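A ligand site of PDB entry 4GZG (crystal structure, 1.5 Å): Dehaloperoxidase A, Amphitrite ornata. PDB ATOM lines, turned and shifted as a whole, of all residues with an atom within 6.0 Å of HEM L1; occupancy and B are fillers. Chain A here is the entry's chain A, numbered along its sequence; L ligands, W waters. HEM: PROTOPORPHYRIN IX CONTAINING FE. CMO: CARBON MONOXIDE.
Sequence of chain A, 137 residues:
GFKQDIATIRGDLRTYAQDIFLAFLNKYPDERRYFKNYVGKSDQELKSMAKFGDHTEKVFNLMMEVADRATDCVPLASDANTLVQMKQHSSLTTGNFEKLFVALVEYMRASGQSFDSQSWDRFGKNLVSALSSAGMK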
ATOM      1  N   PHE A  24      10.877   1.878   8.022  1.00  0.00           N
ATOM      2  CA  PHE A  24      12.062   1.260   7.483  1.00  0.00           C
ATOM      3  C   PHE A  24      13.360   1.858   7.951  1.00  0.00           C
ATOM      4  O   PHE A  24      14.256   1.174   8.473  1.00  0.00           O
ATOM      5  CB  PHE A  24      11.938   1.275   5.935  1.00  0.00           C
ATOM      6  CG  PHE A  24      13.164   0.889   5.202  1.00  0.00           C
ATOM      7  CD1 PHE A  24      13.800  -0.339   5.410  1.00  0.00           C
ATOM      8  CD2 PHE A  24      13.668   1.778   4.273  1.00  0.00           C
ATOM      9  CE1 PHE A  24      14.932  -0.727   4.655  1.00  0.00           C
ATOM     10  CE2 PHE A  24      14.840   1.401   3.492  1.00  0.00           C
ATOM     11  CZ  PHE A  24      15.413   0.170   3.700  1.00  0.00           C
ATOM     12  N   GLU A  31      20.397   2.169   6.715  1.00  0.00           N
ATOM     13  CA  GLU A  31      19.870   2.276   5.384  1.00  0.00           C
ATOM     14  C   GLU A  31      19.697   3.720   4.940  1.00  0.00           C
ATOM     15  O   GLU A  31      19.635   3.958   3.818  1.00  0.00           O
ATOM     16  CB  GLU A  31      18.497   1.529   5.237  1.00  0.00           C
ATOM     17  CG  GLU A  31      18.539   0.009   5.428  1.00  0.00           C
ATOM     18  CD  GLU A  31      19.282  -0.685   4.325  1.00  0.00           C
ATOM     19  OE1 GLU A  31      20.335  -1.158   4.631  1.00  0.00           O
ATOM     20  OE2 GLU A  31      18.892  -0.680   3.251  1.00  0.00           O
ATOM     21  N   TYR A  34      21.901   5.509   2.090  1.00  0.00           N
ATOM     22  CA  TYR A  34      21.650   5.472   0.684  1.00  0.00           C
ATOM     23  C   TYR A  34      20.874   6.700   0.167  1.00  0.00           C
ATOM     24  O   TYR A  34      20.753   6.908  -1.063  1.00  0.00           O
ATOM     25  CB  TYR A  34      20.879   4.211   0.340  1.00  0.00           C
ATOM     26  CG  TYR A  34      21.576   2.949   0.520  1.00  0.00           C
ATOM     27  CD1 TYR A  34      22.522   2.493  -0.415  1.00  0.00           C
ATOM     28  CD2 TYR A  34      21.274   2.150   1.586  1.00  0.00           C
ATOM     29  CE1 TYR A  34      23.192   1.280  -0.203  1.00  0.00           C
ATOM     30  CE2 TYR A  34      21.936   0.947   1.804  1.00  0.00           C
ATOM     31  CZ  TYR A  34      22.882   0.545   0.900  1.00  0.00           C
ATOM     32  OH  TYR A  34      23.493  -0.663   1.076  1.00  0.00           O
ATOM     33  N   PHE A  35      20.366   7.536   1.098  1.00  0.00           N
ATOM     34  CA  PHE A  35      19.539   8.665   0.813  1.00  0.00           C
ATOM     35  C   PHE A  35      20.254   9.873   1.423  1.00  0.00           C
ATOM     36  O   PHE A  35      19.934  10.328   2.531  1.00  0.00           O
ATOM     37  CB  PHE A  35      18.166   8.436   1.517  1.00  0.00           C
ATOM     38  CG  PHE A  35      17.451   7.224   1.019  1.00  0.00           C
ATOM     39  CD1 PHE A  35      17.621   6.037   1.697  1.00  0.00           C
ATOM     40  CD2 PHE A  35      16.635   7.247  -0.079  1.00  0.00           C
ATOM     41  CE1 PHE A  35      16.991   4.858   1.273  1.00  0.00           C
ATOM     42  CE2 PHE A  35      15.985   6.071  -0.472  1.00  0.00           C
ATOM     43  CZ  PHE A  35      16.168   4.931   0.185  1.00  0.00           C
ATOM     44  N   TYR A  38      18.780  12.898   3.275  1.00  0.00           N
ATOM     45  CA  TYR A  38      17.886  12.702   4.454  1.00  0.00           C
ATOM     46  C   TYR A  38      18.693  12.516   5.715  1.00  0.00           C
ATOM     47  O   TYR A  38      18.125  12.359   6.803  1.00  0.00           O
ATOM     48  CB  TYR A  38      16.970  11.467   4.272  1.00  0.00           C
ATOM     49  CG  TYR A  38      16.064  11.524   3.059  1.00  0.00           C
ATOM     50  CD1 TYR A  38      15.828  12.712   2.357  1.00  0.00           C
ATOM     51  CD2 TYR A  38      15.530  10.355   2.587  1.00  0.00           C
ATOM     52  CE1 TYR A  38      15.027  12.708   1.194  1.00  0.00           C
ATOM     53  CE2 TYR A  38      14.723  10.356   1.455  1.00  0.00           C
ATOM     54  CZ  TYR A  38      14.507  11.517   0.788  1.00  0.00           C
ATOM     55  OH  TYR A  38      13.738  11.491  -0.365  1.00  0.00           O
ATOM     56  N   LYS A  51      11.343  16.908  -2.161  1.00  0.00           N
ATOM     57  CA  LYS A  51      11.777  15.638  -2.739  1.00  0.00           C
ATOM     58  C   LYS A  51      11.434  14.453  -1.881  1.00  0.00           C
ATOM     59  O   LYS A  51      11.219  13.344  -2.377  1.00  0.00           O
ATOM     60  CB  LYS A  51      13.291  15.595  -3.043  1.00  0.00           C
ATOM     61  CG  LYS A  51      13.552  15.879  -4.545  1.00  0.00           C
ATOM     62  CD  LYS A  51      14.907  16.296  -4.951  1.00  0.00           C
ATOM     63  CE  LYS A  51      14.787  16.963  -6.369  1.00  0.00           C
ATOM     64  NZ  LYS A  51      16.064  17.127  -7.177  1.00  0.00           N
ATOM     65  N   ASP A  54       7.709  13.788  -2.402  1.00  0.00           N
ATOM     66  CA  ASP A  54       7.432  13.504  -3.771  1.00  0.00           C
ATOM     67  C   ASP A  54       8.116  12.164  -4.150  1.00  0.00           C
ATOM     68  O   ASP A  54       7.429  11.310  -4.735  1.00  0.00           O
ATOM     69  CB  ASP A  54       7.708  14.744  -4.656  1.00  0.00           C
ATOM     70  CG  ASP A  54       6.912  15.998  -4.184  1.00  0.00           C
ATOM     71  OD1 ASP A  54       7.430  17.151  -4.288  1.00  0.00           O
ATOM     72  OD2 ASP A  54       5.782  15.840  -3.674  1.00  0.00           O
ATOM     73  N   HIS A  55       9.373  11.934  -3.788  1.00  0.00           N
ATOM     74  CA  HIS A  55      10.078  10.743  -4.191  1.00  0.00           C
ATOM     75  C   HIS A  55       9.553   9.527  -3.332  1.00  0.00           C
ATOM     76  O   HIS A  55       9.336   8.447  -3.918  1.00  0.00           O
ATOM     77  CB  HIS A  55      11.630  10.968  -4.132  1.00  0.00           C
ATOM     78  CG  HIS A  55      12.148  11.982  -5.119  1.00  0.00           C
ATOM     79  ND1 HIS A  55      13.501  12.116  -5.406  1.00  0.00           N
ATOM     80  CD2 HIS A  55      11.508  12.851  -5.954  1.00  0.00           C
ATOM     81  CE1 HIS A  55      13.657  13.032  -6.352  1.00  0.00           C
ATOM     82  NE2 HIS A  55      12.463  13.533  -6.662  1.00  0.00           N
ATOM     83  N   THR A  56       9.134   9.646  -2.060  1.00  0.00           N
ATOM     84  CA  THR A  56       8.579   8.500  -1.311  1.00  0.00           C
ATOM     85  C   THR A  56       7.244   8.118  -1.878  1.00  0.00           C
ATOM     86  O   THR A  56       6.926   6.935  -1.966  1.00  0.00           O
ATOM     87  CB  THR A  56       8.251   8.684   0.240  1.00  0.00           C
ATOM     88  OG1 THR A  56       7.424   9.822   0.490  1.00  0.00           O
ATOM     89  CG2 THR A  56       9.444   8.704   1.136  1.00  0.00           C
ATOM     90  N   LYS A  58       6.359   8.373  -4.997  1.00  0.00           N
ATOM     91  CA  LYS A  58       6.730   7.679  -6.215  1.00  0.00           C
ATOM     92  C   LYS A  58       7.208   6.276  -5.984  1.00  0.00           C
ATOM     93  O   LYS A  58       6.819   5.370  -6.762  1.00  0.00           O
ATOM     94  CB  LYS A  58       7.695   8.521  -7.095  1.00  0.00           C
ATOM     95  CG  LYS A  58       6.866   9.748  -7.678  1.00  0.00           C
ATOM     96  CD  LYS A  58       7.677  10.798  -8.458  1.00  0.00           C
ATOM     97  CE  LYS A  58       6.650  11.972  -8.876  1.00  0.00           C
ATOM     98  NZ  LYS A  58       7.464  13.056  -9.396  1.00  0.00           N
ATOM     99  N   VAL A  59       8.039   6.082  -4.939  1.00  0.00           N
ATOM    100  CA  VAL A  59       8.440   4.711  -4.592  1.00  0.00           C
ATOM    101  C   VAL A  59       7.199   3.855  -4.325  1.00  0.00           C
ATOM    102  O   VAL A  59       7.065   2.727  -4.843  1.00  0.00           O
ATOM    103  CB  VAL A  59       9.221   4.801  -3.304  1.00  0.00           C
ATOM    104  CG1 VAL A  59       9.463   3.401  -2.671  1.00  0.00           C
ATOM    105  CG2 VAL A  59      10.540   5.505  -3.589  1.00  0.00           C
ATOM    106  N   PHE A  60       6.282   4.315  -3.512  1.00  0.00           N
ATOM    107  CA  PHE A  60       5.148   3.518  -3.106  1.00  0.00           C
ATOM    108  C   PHE A  60       4.152   3.394  -4.216  1.00  0.00           C
ATOM    109  O   PHE A  60       3.424   2.399  -4.253  1.00  0.00           O
ATOM    110  CB  PHE A  60       4.546   3.895  -1.735  1.00  0.00           C
ATOM    111  CG  PHE A  60       5.418   3.402  -0.618  1.00  0.00           C
ATOM    112  CD1 PHE A  60       5.064   2.222   0.050  1.00  0.00           C
ATOM    113  CD2 PHE A  60       6.636   4.044  -0.315  1.00  0.00           C
ATOM    114  CE1 PHE A  60       5.895   1.713   1.030  1.00  0.00           C
ATOM    115  CE2 PHE A  60       7.491   3.536   0.709  1.00  0.00           C
ATOM    116  CZ  PHE A  60       7.071   2.358   1.354  1.00  0.00           C
ATOM    117  N   LEU A  62       4.984   3.003  -7.415  1.00  0.00           N
ATOM    118  CA  LEU A  62       5.544   1.895  -8.133  1.00  0.00           C
ATOM    119  C   LEU A  62       5.334   0.570  -7.319  1.00  0.00           C
ATOM    120  O   LEU A  62       4.946  -0.439  -7.961  1.00  0.00           O
ATOM    121  CB  LEU A  62       7.002   2.120  -8.482  1.00  0.00           C
ATOM    122  CG  LEU A  62       7.618   0.971  -9.345  1.00  0.00           C
ATOM    123  CD1 LEU A  62       6.861   0.613 -10.642  1.00  0.00           C
ATOM    124  CD2 LEU A  62       9.063   1.297  -9.643  1.00  0.00           C
ATOM    125  N   MET A  63       5.547   0.546  -5.996  1.00  0.00           N
ATOM    126  CA  MET A  63       5.308  -0.717  -5.277  1.00  0.00           C
ATOM    127  C   MET A  63       3.871  -1.202  -5.501  1.00  0.00           C
ATOM    128  O   MET A  63       3.612  -2.398  -5.605  1.00  0.00           O
ATOM    129  CB  MET A  63       5.522  -0.439  -3.796  1.00  0.00           C
ATOM    130  CG  MET A  63       5.546  -1.794  -3.087  1.00  0.00           C
ATOM    131  SD  MET A  63       5.679  -1.661  -1.254  1.00  0.00           S
ATOM    132  CE  MET A  63       7.308  -0.969  -1.134  1.00  0.00           C
ATOM    133  N   VAL A  66       3.385  -2.732  -8.898  1.00  0.00           N
ATOM    134  CA  VAL A  66       3.949  -4.091  -8.929  1.00  0.00           C
ATOM    135  C   VAL A  66       3.030  -5.034  -8.133  1.00  0.00           C
ATOM    136  O   VAL A  66       2.695  -6.141  -8.598  1.00  0.00           O
ATOM    137  CB  VAL A  66       5.326  -4.045  -8.372  1.00  0.00           C
ATOM    138  CG1 VAL A  66       5.908  -5.530  -8.290  1.00  0.00           C
ATOM    139  CG2 VAL A  66       6.257  -3.170  -9.268  1.00  0.00           C
ATOM    140  N   LEU A  83      13.004  -2.818 -11.351  1.00  0.00           N
ATOM    141  CA  LEU A  83      13.526  -2.384 -10.091  1.00  0.00           C
ATOM    142  C   LEU A  83      15.054  -2.631 -10.037  1.00  0.00           C
ATOM    143  O   LEU A  83      15.838  -1.858  -9.458  1.00  0.00           O
ATOM    144  CB  LEU A  83      12.894  -3.155  -8.943  1.00  0.00           C
ATOM    145  CG  LEU A  83      11.433  -2.802  -8.792  1.00  0.00           C
ATOM    146  CD1 LEU A  83      10.785  -3.740  -7.743  1.00  0.00           C
ATOM    147  CD2 LEU A  83      11.257  -1.376  -8.314  1.00  0.00           C
ATOM    148  N   MET A  86      16.975   0.063 -12.492  1.00  0.00           N
ATOM    149  CA  MET A  86      16.947   1.517 -12.113  1.00  0.00           C
ATOM    150  C   MET A  86      18.309   1.956 -11.671  1.00  0.00           C
ATOM    151  O   MET A  86      18.873   1.322 -10.813  1.00  0.00           O
ATOM    152  CB  MET A  86      16.024   1.718 -10.918  1.00  0.00           C
ATOM    153  CG  MET A  86      14.630   1.568 -11.284  1.00  0.00           C
ATOM    154  SD  MET A  86      13.477   1.878  -9.955  1.00  0.00           S
ATOM    155  CE  MET A  86      14.182   3.262  -9.063  1.00  0.00           C
ATOM    156  N   GLN A  88      19.056   4.289  -9.827  1.00  0.00           N
ATOM    157  CA  GLN A  88      19.002   4.606  -8.400  1.00  0.00           C
ATOM    158  C   GLN A  88      19.190   3.372  -7.524  1.00  0.00           C
ATOM    159  O   GLN A  88      19.436   3.475  -6.314  1.00  0.00           O
ATOM    160  CB  GLN A  88      17.664   5.226  -8.040  1.00  0.00           C
ATOM    161  CG  GLN A  88      17.277   6.511  -8.766  1.00  0.00           C
ATOM    162  CD  GLN A  88      16.419   6.193  -9.972  1.00  0.00           C
ATOM    163  OE1 GLN A  88      16.675   5.229 -10.760  1.00  0.00           O
ATOM    164  NE2 GLN A  88      15.405   7.023 -10.167  1.00  0.00           N
ATOM    165  N   HIS A  89      19.008   2.159  -8.104  1.00  0.00           N
ATOM    166  CA  HIS A  89      19.160   0.946  -7.304  1.00  0.00           C
ATOM    167  C   HIS A  89      20.426   0.197  -7.628  1.00  0.00           C
ATOM    168  O   HIS A  89      20.566  -0.937  -7.216  1.00  0.00           O
ATOM    169  CB  HIS A  89      17.920   0.031  -7.559  1.00  0.00           C
ATOM    170  CG  HIS A  89      16.604   0.614  -7.029  1.00  0.00           C
ATOM    171  ND1 HIS A  89      15.404   0.143  -7.465  1.00  0.00           N
ATOM    172  CD2 HIS A  89      16.314   1.535  -6.068  1.00  0.00           C
ATOM    173  CE1 HIS A  89      14.419   0.719  -6.784  1.00  0.00           C
ATOM    174  NE2 HIS A  89      14.934   1.615  -5.956  1.00  0.00           N
ATOM    175  N   LEU A  92      22.417  -1.642  -4.770  1.00  0.00           N
ATOM    176  CA  LEU A  92      21.677  -2.463  -3.776  1.00  0.00           C
ATOM    177  C   LEU A  92      21.796  -3.933  -4.002  1.00  0.00           C
ATOM    178  O   LEU A  92      22.235  -4.438  -5.042  1.00  0.00           O
ATOM    179  CB  LEU A  92      20.174  -2.067  -3.755  1.00  0.00           C
ATOM    180  CG  LEU A  92      19.818  -0.566  -3.732  1.00  0.00           C
ATOM    181  CD1 LEU A  92      18.243  -0.412  -3.832  1.00  0.00           C
ATOM    182  CD2 LEU A  92      20.432   0.065  -2.474  1.00  0.00           C
ATOM    183  N   ASN A  96      18.599  -5.438   0.950  1.00  0.00           N
ATOM    184  CA  ASN A  96      18.001  -4.111   1.182  1.00  0.00           C
ATOM    185  C   ASN A  96      16.487  -4.176   1.062  1.00  0.00           C
ATOM    186  O   ASN A  96      15.771  -3.581   1.870  1.00  0.00           O
ATOM    187  CB  ASN A  96      18.576  -3.022   0.250  1.00  0.00           C
ATOM    188  CG  ASN A  96      20.051  -2.864   0.415  1.00  0.00           C
ATOM    189  OD1 ASN A  96      20.795  -3.327  -0.442  1.00  0.00           O
ATOM    190  ND2 ASN A  96      20.467  -2.122   1.356  1.00  0.00           N
ATOM    191  N   PHE A  97      16.037  -4.905   0.059  1.00  0.00           N
ATOM    192  CA  PHE A  97      14.640  -5.120  -0.156  1.00  0.00           C
ATOM    193  C   PHE A  97      14.022  -5.958   0.925  1.00  0.00           C
ATOM    194  O   PHE A  97      12.882  -5.632   1.378  1.00  0.00           O
ATOM    195  CB  PHE A  97      14.397  -5.665  -1.592  1.00  0.00           C
ATOM    196  CG  PHE A  97      14.706  -4.674  -2.670  1.00  0.00           C
ATOM    197  CD1 PHE A  97      13.673  -3.994  -3.356  1.00  0.00           C
ATOM    198  CD2 PHE A  97      16.049  -4.411  -3.049  1.00  0.00           C
ATOM    199  CE1 PHE A  97      13.949  -3.093  -4.360  1.00  0.00           C
ATOM    200  CE2 PHE A  97      16.356  -3.509  -4.031  1.00  0.00           C
ATOM    201  CZ  PHE A  97      15.287  -2.750  -4.633  1.00  0.00           C
ATOM    202  N   LEU A 100      13.303  -3.678   3.821  1.00  0.00           N
ATOM    203  CA  LEU A 100      12.101  -2.837   3.619  1.00  0.00           C
ATOM    204  C   LEU A 100      10.831  -3.643   3.885  1.00  0.00           C
ATOM    205  O   LEU A 100       9.938  -3.150   4.573  1.00  0.00           O
ATOM    206  CB  LEU A 100      12.133  -2.284   2.189  1.00  0.00           C
ATOM    207  CG  LEU A 100      10.860  -1.544   1.724  1.00  0.00           C
ATOM    208  CD1 LEU A 100      10.627  -0.319   2.590  1.00  0.00           C
ATOM    209  CD2 LEU A 100      11.048  -1.142   0.266  1.00  0.00           C
ATOM    210  N   PHE A 101      10.793  -4.877   3.394  1.00  0.00           N
ATOM    211  CA  PHE A 101       9.583  -5.618   3.609  1.00  0.00           C
ATOM    212  C   PHE A 101       9.397  -6.107   5.030  1.00  0.00           C
ATOM    213  O   PHE A 101       8.251  -6.118   5.505  1.00  0.00           O
ATOM    214  CB  PHE A 101       9.463  -6.758   2.546  1.00  0.00           C
ATOM    215  CG  PHE A 101       8.935  -6.233   1.265  1.00  0.00           C
ATOM    216  CD1 PHE A 101       9.788  -5.846   0.262  1.00  0.00           C
ATOM    217  CD2 PHE A 101       7.597  -6.016   1.095  1.00  0.00           C
ATOM    218  CE1 PHE A 101       9.333  -5.308  -0.947  1.00  0.00           C
ATOM    219  CE2 PHE A 101       7.160  -5.479  -0.058  1.00  0.00           C
ATOM    220  CZ  PHE A 101       8.018  -5.076  -1.080  1.00  0.00           C
ATOM    221  N   LEU A 127       9.172 -11.264  -4.325  1.00  0.00           N
ATOM    222  CA  LEU A 127       9.830 -10.166  -5.029  1.00  0.00           C
ATOM    223  C   LEU A 127      11.322 -10.320  -4.864  1.00  0.00           C
ATOM    224  O   LEU A 127      12.059 -10.105  -5.856  1.00  0.00           O
ATOM    225  CB  LEU A 127       9.339  -8.825  -4.517  1.00  0.00           C
ATOM    226  CG  LEU A 127       9.977  -7.613  -5.273  1.00  0.00           C
ATOM    227  CD1 LEU A 127       9.666  -7.608  -6.721  1.00  0.00           C
ATOM    228  CD2 LEU A 127       9.491  -6.294  -4.707  1.00  0.00           C
HETATM  229  CHA HEM L   1      14.564   5.726  -5.941  1.00  0.00           C
HETATM  230  CHB HEM L   1      11.059   2.410  -6.212  1.00  0.00           C
HETATM  231  CHC HEM L   1      13.235  -0.243  -2.815  1.00  0.00           C
HETATM  232  CHD HEM L   1      16.899   2.897  -2.626  1.00  0.00           C
HETATM  233  C1A HEM L   1      13.402   5.125  -6.296  1.00  0.00           C
HETATM  234  C2A HEM L   1      12.372   5.560  -7.189  1.00  0.00           C
HETATM  235  C3A HEM L   1      11.408   4.679  -7.303  1.00  0.00           C
HETATM  236  C4A HEM L   1      11.809   3.594  -6.438  1.00  0.00           C
HETATM  237  CMA HEM L   1      10.141   4.789  -8.161  1.00  0.00           C
HETATM  238  CAA HEM L   1      12.418   6.888  -7.985  1.00  0.00           C
HETATM  239  CBA HEM L   1      11.907   8.018  -7.100  1.00  0.00           C
HETATM  240  CGA HEM L   1      11.962   9.379  -7.778  1.00  0.00           C
HETATM  241  O1A HEM L   1      11.017  10.175  -7.593  1.00  0.00           O
HETATM  242  O2A HEM L   1      12.953   9.734  -8.457  1.00  0.00           O
HETATM  243  C1B HEM L   1      11.356   1.411  -5.311  1.00  0.00           C
HETATM  244  C2B HEM L   1      10.500   0.345  -5.009  1.00  0.00           C
HETATM  245  C3B HEM L   1      11.117  -0.392  -4.103  1.00  0.00           C
HETATM  246  C4B HEM L   1      12.355   0.235  -3.737  1.00  0.00           C
HETATM  247  CMB HEM L   1       9.168   0.115  -5.624  1.00  0.00           C
HETATM  248  CAB HEM L   1      10.595  -1.691  -3.426  1.00  0.00           C
HETATM  249  CBB HEM L   1       9.789  -2.605  -3.995  1.00  0.00           C
HETATM  250  C1C HEM L   1      14.389   0.371  -2.444  1.00  0.00           C
HETATM  251  C2C HEM L   1      15.244  -0.012  -1.356  1.00  0.00           C
HETATM  252  C3C HEM L   1      16.257   0.862  -1.294  1.00  0.00           C
HETATM  253  C4C HEM L   1      16.054   1.834  -2.358  1.00  0.00           C
HETATM  254  CMC HEM L   1      14.989  -1.219  -0.509  1.00  0.00           C
HETATM  255  CAC HEM L   1      17.435   0.963  -0.303  1.00  0.00           C
HETATM  256  CBC HEM L   1      17.592   0.389   0.875  1.00  0.00           C
HETATM  257  C1D HEM L   1      16.596   3.959  -3.457  1.00  0.00           C
HETATM  258  C2D HEM L   1      17.400   5.127  -3.653  1.00  0.00           C
HETATM  259  C3D HEM L   1      16.742   6.023  -4.610  1.00  0.00           C
HETATM  260  C4D HEM L   1      15.545   5.291  -5.048  1.00  0.00           C
HETATM  261  CMD HEM L   1      18.655   5.361  -2.865  1.00  0.00           C
HETATM  262  CAD HEM L   1      17.175   7.373  -5.092  1.00  0.00           C
HETATM  263  CBD HEM L   1      16.684   8.463  -4.079  1.00  0.00           C
HETATM  264  CGD HEM L   1      15.909   9.653  -4.678  1.00  0.00           C
HETATM  265  O1D HEM L   1      16.450  10.285  -5.632  1.00  0.00           O
HETATM  266  O2D HEM L   1      14.783  10.044  -4.210  1.00  0.00           O
HETATM  267  NA  HEM L   1      13.015   3.909  -5.798  1.00  0.00           N
HETATM  268  NB  HEM L   1      12.478   1.342  -4.496  1.00  0.00           N
HETATM  269  NC  HEM L   1      14.912   1.502  -3.044  1.00  0.00           N
HETATM  270  ND  HEM L   1      15.506   4.027  -4.337  1.00  0.00           N
HETATM  271 FE   HEM L   1      13.993   2.686  -4.456  1.00  0.00          FE
HETATM  272  C   CMO L   2      13.231   3.761  -2.691  1.00  0.00           C
HETATM  273  O   CMO L   2      12.873   4.002  -1.673  1.00  0.00           O
HETATM  274  O   HOH W   1      11.051  12.171  -9.278  1.00  0.00           O
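A ring nitrogen (ND1) of His 55 lies within hydrogen-bond range of an oxygen (O2D) of HEM L1 (2.7 Å).
FE of HEM L1 is bound by NE2 of His 89 (2.1 Å).
OE2 of Glu 31 is in hydrogen-bond range of ND2 of Asn 96.
OH of Tyr 34 is in hydrogen-bond range of ND2 of Asn 96, 3.4 Å away.
A ring nitrogen (ND1) of His 89 lies close to the side-chain sulfur (SD) of Met 86, 3.6 Å away.
A ring nitrogen (ND1) of His 89 is in hydrogen-bond range of the backbone carbonyl oxygen of Leu 83 (2.9 Å).
Merely in contact with HEM L1: Phe 24, Glu 31, Tyr 34, Phe 35, Lys 58, Val 59, Leu 62, Met 63, Leu 83, Met 86, Gln 88, Leu 92, Asn 96, Phe 97, Leu 100 and Leu 127.
Hydrophobic or aromatic side chains within 4 Å of HEM L1: Phe 24, Phe 35, His 55, Val 59, Leu 62, Leu 83, Met 86, His 89, Leu 92, Phe 97, Leu 100 and Leu 127.
18 residues have an atom within 4 Å of HEM L1: Phe 24, Glu 31, Tyr 34, Phe 35, His 55, Lys 58, Val 59, Leu 62, Met 63, Leu 83, Met 86, Gln 88, His 89, Leu 92, Asn 96, Phe 97, Leu 100 and Leu 127.
Water W1 lies within hydrogen-bond range of O1A of HEM L1 and NE2 of His 55.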
